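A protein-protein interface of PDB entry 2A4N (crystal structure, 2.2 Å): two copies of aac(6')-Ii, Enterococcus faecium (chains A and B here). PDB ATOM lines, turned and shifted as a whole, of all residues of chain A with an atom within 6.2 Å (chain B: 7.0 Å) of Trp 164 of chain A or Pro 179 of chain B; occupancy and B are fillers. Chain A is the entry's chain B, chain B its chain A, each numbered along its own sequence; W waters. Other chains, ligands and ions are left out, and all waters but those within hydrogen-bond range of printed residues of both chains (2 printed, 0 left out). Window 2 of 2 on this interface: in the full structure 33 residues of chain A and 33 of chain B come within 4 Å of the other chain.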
ATOM      1  N   GLN A 122      31.577  16.080  -8.441  1.00  0.00           N
ATOM      2  CA  GLN A 122      30.863  15.201  -7.519  1.00  0.00           C
ATOM      3  C   GLN A 122      30.773  15.766  -6.098  1.00  0.00           C
ATOM      4  O   GLN A 122      30.843  15.025  -5.113  1.00  0.00           O
ATOM      5  CB  GLN A 122      31.520  13.819  -7.491  1.00  0.00           C
ATOM      6  CG  GLN A 122      31.789  13.253  -8.876  1.00  0.00           C
ATOM      7  CD  GLN A 122      31.339  11.811  -9.034  1.00  0.00           C
ATOM      8  OE1 GLN A 122      31.549  10.977  -8.147  1.00  0.00           O
ATOM      9  NE2 GLN A 122      30.726  11.506 -10.176  1.00  0.00           N
ATOM     10  N   ASN A 160      28.268  23.221 -11.499  1.00  0.00           N
ATOM     11  CA  ASN A 160      27.191  22.600 -12.265  1.00  0.00           C
ATOM     12  C   ASN A 160      27.057  23.069 -13.706  1.00  0.00           C
ATOM     13  O   ASN A 160      25.949  23.090 -14.251  1.00  0.00           O
ATOM     14  CB  ASN A 160      25.868  22.840 -11.538  1.00  0.00           C
ATOM     15  CG  ASN A 160      25.985  22.614 -10.044  1.00  0.00           C
ATOM     16  OD1 ASN A 160      26.421  21.552  -9.602  1.00  0.00           O
ATOM     17  ND2 ASN A 160      25.601  23.614  -9.257  1.00  0.00           N
ATOM     18  N   ALA A 161      28.175  23.432 -14.322  1.00  0.00           N
ATOM     19  CA  ALA A 161      28.178  23.903 -15.697  1.00  0.00           C
ATOM     20  C   ALA A 161      27.615  22.905 -16.714  1.00  0.00           C
ATOM     21  O   ALA A 161      26.759  23.252 -17.529  1.00  0.00           O
ATOM     22  CB  ALA A 161      29.593  24.294 -16.095  1.00  0.00           C
ATOM     23  N   ASN A 162      28.094  21.668 -16.647  1.00  0.00           N
ATOM     24  CA  ASN A 162      27.704  20.603 -17.573  1.00  0.00           C
ATOM     25  C   ASN A 162      26.717  19.617 -16.947  1.00  0.00           C
ATOM     26  O   ASN A 162      26.607  18.482 -17.398  1.00  0.00           O
ATOM     27  CB  ASN A 162      28.955  19.824 -17.986  1.00  0.00           C
ATOM     28  CG  ASN A 162      30.030  20.710 -18.558  1.00  0.00           C
ATOM     29  OD1 ASN A 162      29.992  21.069 -19.732  1.00  0.00           O
ATOM     30  ND2 ASN A 162      30.994  21.086 -17.723  1.00  0.00           N
ATOM     31  N   GLY A 163      26.014  20.050 -15.911  1.00  0.00           N
ATOM     32  CA  GLY A 163      25.088  19.171 -15.216  1.00  0.00           C
ATOM     33  C   GLY A 163      25.535  19.187 -13.767  1.00  0.00           C
ATOM     34  O   GLY A 163      26.659  19.605 -13.482  1.00  0.00           O
ATOM     35  N   TRP A 164      24.692  18.737 -12.848  1.00  0.00           N
ATOM     36  CA  TRP A 164      25.071  18.765 -11.438  1.00  0.00           C
ATOM     37  C   TRP A 164      26.440  18.159 -11.145  1.00  0.00           C
ATOM     38  O   TRP A 164      26.757  17.053 -11.588  1.00  0.00           O
ATOM     39  CB  TRP A 164      24.001  18.079 -10.580  1.00  0.00           C
ATOM     40  CG  TRP A 164      22.676  18.796 -10.618  1.00  0.00           C
ATOM     41  CD1 TRP A 164      21.605  18.511 -11.422  1.00  0.00           C
ATOM     42  CD2 TRP A 164      22.304  19.943  -9.845  1.00  0.00           C
ATOM     43  NE1 TRP A 164      20.588  19.410 -11.193  1.00  0.00           N
ATOM     44  CE2 TRP A 164      20.989  20.299 -10.231  1.00  0.00           C
ATOM     45  CE3 TRP A 164      22.953  20.707  -8.862  1.00  0.00           C
ATOM     46  CZ2 TRP A 164      20.312  21.384  -9.667  1.00  0.00           C
ATOM     47  CZ3 TRP A 164      22.279  21.787  -8.302  1.00  0.00           C
ATOM     48  CH2 TRP A 164      20.970  22.114  -8.708  1.00  0.00           C
ATOM     49  N   ASP A 165      27.251  18.912 -10.404  1.00  0.00           N
ATOM     50  CA  ASP A 165      28.588  18.493 -10.006  1.00  0.00           C
ATOM     51  C   ASP A 165      29.546  18.138 -11.147  1.00  0.00           C
ATOM     52  O   ASP A 165      30.419  17.286 -10.991  1.00  0.00           O
ATOM     53  CB  ASP A 165      28.495  17.326  -9.016  1.00  0.00           C
ATOM     54  CG  ASP A 165      27.744  17.696  -7.749  1.00  0.00           C
ATOM     55  OD1 ASP A 165      27.420  18.893  -7.576  1.00  0.00           O
ATOM     56  OD2 ASP A 165      27.480  16.796  -6.920  1.00  0.00           O
ATOM     57  N   LYS A 166      29.367  18.791 -12.293  1.00  0.00           N
ATOM     58  CA  LYS A 166      30.234  18.613 -13.462  1.00  0.00           C
ATOM     59  C   LYS A 166      30.596  20.044 -13.845  1.00  0.00           C
ATOM     60  O   LYS A 166      30.084  20.612 -14.808  1.00  0.00           O
ATOM     61  CB  LYS A 166      29.494  17.912 -14.604  1.00  0.00           C
ATOM     62  CG  LYS A 166      29.061  16.486 -14.263  1.00  0.00           C
ATOM     63  CD  LYS A 166      28.398  15.793 -15.444  1.00  0.00           C
ATOM     64  CE  LYS A 166      27.963  14.379 -15.075  1.00  0.00           C
ATOM     65  NZ  LYS A 166      29.110  13.569 -14.609  1.00  0.00           N
ATOM     66  N   PRO A 167      31.504  20.648 -13.078  1.00  0.00           N
ATOM     67  CA  PRO A 167      31.950  22.022 -13.292  1.00  0.00           C
ATOM     68  C   PRO A 167      32.940  22.260 -14.419  1.00  0.00           C
ATOM     69  O   PRO A 167      33.473  21.331 -15.019  1.00  0.00           O
ATOM     70  CB  PRO A 167      32.569  22.373 -11.953  1.00  0.00           C
ATOM     71  CG  PRO A 167      33.315  21.089 -11.637  1.00  0.00           C
ATOM     72  CD  PRO A 167      32.288  20.001 -12.005  1.00  0.00           C
ATOM     73  N   THR B  69      22.528  22.701 -19.871  1.00  0.00           N
ATOM     74  CA  THR B  69      22.667  22.962 -18.443  1.00  0.00           C
ATOM     75  C   THR B  69      23.221  24.329 -18.043  1.00  0.00           C
ATOM     76  O   THR B  69      22.764  24.924 -17.059  1.00  0.00           O
ATOM     77  CB  THR B  69      23.556  21.893 -17.796  1.00  0.00           C
ATOM     78  OG1 THR B  69      24.804  21.833 -18.503  1.00  0.00           O
ATOM     79  CG2 THR B  69      22.860  20.517 -17.844  1.00  0.00           C
ATOM     80  N   ILE B 105      20.336  24.613 -15.761  1.00  0.00           N
ATOM     81  CA  ILE B 105      20.625  24.509 -14.330  1.00  0.00           C
ATOM     82  C   ILE B 105      21.375  25.714 -13.762  1.00  0.00           C
ATOM     83  O   ILE B 105      21.074  26.184 -12.667  1.00  0.00           O
ATOM     84  CB  ILE B 105      21.466  23.235 -14.050  1.00  0.00           C
ATOM     85  CG1 ILE B 105      20.582  21.997 -14.185  1.00  0.00           C
ATOM     86  CG2 ILE B 105      22.106  23.298 -12.671  1.00  0.00           C
ATOM     87  CD1 ILE B 105      21.342  20.701 -13.982  1.00  0.00           C
ATOM     88  N   THR B 174      22.811  28.766  -9.540  1.00  0.00           N
ATOM     89  CA  THR B 174      22.108  27.575  -9.989  1.00  0.00           C
ATOM     90  C   THR B 174      20.656  27.929  -9.732  1.00  0.00           C
ATOM     91  O   THR B 174      20.267  28.232  -8.608  1.00  0.00           O
ATOM     92  CB  THR B 174      22.547  26.344  -9.189  1.00  0.00           C
ATOM     93  OG1 THR B 174      23.876  25.983  -9.593  1.00  0.00           O
ATOM     94  CG2 THR B 174      21.607  25.177  -9.434  1.00  0.00           C
ATOM     95  N   ILE B 175      19.859  27.895 -10.789  1.00  0.00           N
ATOM     96  CA  ILE B 175      18.467  28.309 -10.714  1.00  0.00           C
ATOM     97  C   ILE B 175      17.356  27.322 -10.364  1.00  0.00           C
ATOM     98  O   ILE B 175      16.185  27.617 -10.597  1.00  0.00           O
ATOM     99  CB  ILE B 175      18.088  29.010 -12.013  1.00  0.00           C
ATOM    100  CG1 ILE B 175      18.202  28.029 -13.181  1.00  0.00           C
ATOM    101  CG2 ILE B 175      19.017  30.196 -12.230  1.00  0.00           C
ATOM    102  CD1 ILE B 175      17.638  28.567 -14.464  1.00  0.00           C
ATOM    103  N   ILE B 176      17.706  26.165  -9.815  1.00  0.00           N
ATOM    104  CA  ILE B 176      16.700  25.185  -9.418  1.00  0.00           C
ATOM    105  C   ILE B 176      17.202  24.420  -8.203  1.00  0.00           C
ATOM    106  O   ILE B 176      18.402  24.368  -7.953  1.00  0.00           O
ATOM    107  CB  ILE B 176      16.369  24.197 -10.558  1.00  0.00           C
ATOM    108  CG1 ILE B 176      17.648  23.537 -11.080  1.00  0.00           C
ATOM    109  CG2 ILE B 176      15.623  24.921 -11.669  1.00  0.00           C
ATOM    110  CD1 ILE B 176      17.402  22.471 -12.137  1.00  0.00           C
ATOM    111  N   PRO B 177      16.288  23.823  -7.421  1.00  0.00           N
ATOM    112  CA  PRO B 177      16.700  23.072  -6.230  1.00  0.00           C
ATOM    113  C   PRO B 177      17.752  22.010  -6.534  1.00  0.00           C
ATOM    114  O   PRO B 177      17.726  21.371  -7.582  1.00  0.00           O
ATOM    115  CB  PRO B 177      15.388  22.455  -5.736  1.00  0.00           C
ATOM    116  CG  PRO B 177      14.357  23.449  -6.189  1.00  0.00           C
ATOM    117  CD  PRO B 177      14.825  23.779  -7.590  1.00  0.00           C
ATOM    118  N   ARG B 178      18.688  21.839  -5.613  1.00  0.00           N
ATOM    119  CA  ARG B 178      19.723  20.837  -5.783  1.00  0.00           C
ATOM    120  C   ARG B 178      19.117  19.474  -5.436  1.00  0.00           C
ATOM    121  O   ARG B 178      18.306  19.352  -4.510  1.00  0.00           O
ATOM    122  CB  ARG B 178      20.916  21.148  -4.869  1.00  0.00           C
ATOM    123  CG  ARG B 178      22.053  20.136  -4.934  1.00  0.00           C
ATOM    124  CD  ARG B 178      23.143  20.474  -3.924  1.00  0.00           C
ATOM    125  NE  ARG B 178      24.154  19.425  -3.866  1.00  0.00           N
ATOM    126  CZ  ARG B 178      25.009  19.142  -4.847  1.00  0.00           C
ATOM    127  NH1 ARG B 178      24.992  19.836  -5.977  1.00  0.00           N
ATOM    128  NH2 ARG B 178      25.879  18.151  -4.696  1.00  0.00           N
ATOM    129  N   PRO B 179      19.469  18.438  -6.203  1.00  0.00           N
ATOM    130  CA  PRO B 179      18.942  17.100  -5.939  1.00  0.00           C
ATOM    131  C   PRO B 179      19.291  16.650  -4.526  1.00  0.00           C
ATOM    132  O   PRO B 179      20.402  16.885  -4.057  1.00  0.00           O
ATOM    133  CB  PRO B 179      19.644  16.253  -6.992  1.00  0.00           C
ATOM    134  CG  PRO B 179      19.750  17.187  -8.138  1.00  0.00           C
ATOM    135  CD  PRO B 179      20.222  18.461  -7.470  1.00  0.00           C
ATOM    136  N   ASP B 180      18.344  16.017  -3.847  1.00  0.00           N
ATOM    137  CA  ASP B 180      18.592  15.524  -2.496  1.00  0.00           C
ATOM    138  C   ASP B 180      17.809  14.235  -2.242  1.00  0.00           C
ATOM    139  O   ASP B 180      17.361  14.022  -1.083  1.00  0.00           O
ATOM    140  CB  ASP B 180      18.195  16.582  -1.457  1.00  0.00           C
ATOM    141  CG  ASP B 180      16.720  16.955  -1.534  1.00  0.00           C
ATOM    142  OD1 ASP B 180      15.866  16.053  -1.700  1.00  0.00           O
ATOM    143  OD2 ASP B 180      16.414  18.160  -1.403  1.00  0.00           O
HETATM  144  O   HOH W   1      25.113  22.949  -6.353  1.00  0.00           O
HETATM  145  O   HOH W   2      25.461  19.722 -20.405  1.00  0.00           O
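The guanidinium group (NH1) of Arg 178 of chain B is in salt-bridge range of the side-chain carboxylate (OD1) of Asp 165 of chain A (3.1 Å). The side-chain hydroxyl of Thr 69 of chain B is in hydrogen-bond range of the backbone NH of Gly 163 of chain A (3.4 Å). OG1 of Thr 174 of chain B sits at hydrogen-bond distance from ND2 of Asn 160 of chain A (2.9 Å). The backbone carbonyl oxygen (O) of Ala 161 of chain A sits at hydrogen-bond distance from the side-chain hydroxyl (OG1) of Thr 69 of chain B, 2.6 Å away.
The backbone NH (N) of Asp 165 of chain A sits at hydrogen-bond distance from the side-chain amide oxygen (OD1) of Asn 160 of chain A, 2.9 Å away. The backbone carbonyl oxygen (O) of Lys 166 of chain A sits at hydrogen-bond distance from the backbone NH (N) of Ala 161 of chain A, at 3.4 Å. The backbone NH (N) of Ile 105 of chain B sits at hydrogen-bond distance from the backbone carbonyl oxygen (O) of Thr 69 of chain B, at 2.8 Å. O of Ile 105 of chain B lies within hydrogen-bond range of N of Ile 175 of chain B (2.8 Å). The backbone carbonyl oxygen of Asp 165 of chain A sits at hydrogen-bond distance from the backbone NH of Gln 122 of chain A (3.0 Å). The backbone carbonyl oxygen (O) of Lys 166 of chain A is in hydrogen-bond range of the side-chain amide nitrogen (ND2) of Asn 162 of chain A, at 3.1 Å.
Among the printed residues, merely in contact across the chains: Asn 160 of chain A with Ile 105 of chain B (3.96 Å), Asn 162 of chain A with Thr 69 of chain B (3.3 Å), Trp 164 of chain A with Ile 105 of chain B (3.2 Å), Trp 164 of chain A with Thr 174 of chain B (3.2 Å), Trp 164 of chain A with Ile 176 of chain B (3.5 Å), Trp 164 of chain A with Pro 177 of chain B (3.3 Å), Trp 164 of chain A with Arg 178 of chain B (3.4 Å) and Trp 164 of chain A with Pro 179 of chain B (3.4 Å).
Of chain B, only Ile 105 (3.2 Å), Thr 174 (3.2 Å), Ile 176 (3.5 Å), Pro 177 (3.3 Å), Arg 178 (3.4 Å) and Pro 179 (3.4 Å) come within 4 Å of Trp 164 of chain A. Pro 179 of chain B touches just one residue of chain A: Trp 164 (3.4 Å). Of the printed residues of chain B, Asp 165 of chain A touches Arg 178 (3.1 Å). Of the printed residues of chain A, Ile 176 of chain B touches Trp 164. Printed residues of chain B within 4 Å of Asn 160 of chain A: Ile 105 (3.96 Å) and Thr 174 (2.9 Å). Printed residues of chain B within 4 Å of Gly 163 of chain A: Thr 69 (3.4 Å). Ile 175 of chain B touches none of the printed residues of chain A. The nearest residue of chain B that does not touch Trp 164 of chain A is Thr 69 of chain B (5.6 Å). The nearest printed residue of chain A that does not touch Pro 179 of chain B is Asp 165 of chain A (7.2 Å).
Among the printed residues, 12 pairs touch across the chains. Among the printed residues, Asp or Glu carboxylates within 4 Å of a Lys or Arg side-chain nitrogen of the other chain: Asp 165 of chain A with Arg 178 of chain B.
No position is printed for both chains.
Water W2 lies within hydrogen-bond range of the side-chain hydroxyl (OG1) of Thr 69 of chain B (2.9 Å) and the backbone carbonyl oxygen (O) of Asn 162 of chain A (3.4 Å). Water W1 lies within hydrogen-bond range of ND2 of Asn 160 of chain A (3.0 Å) and NH1 of Arg 178 of chain B (3.1 Å).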
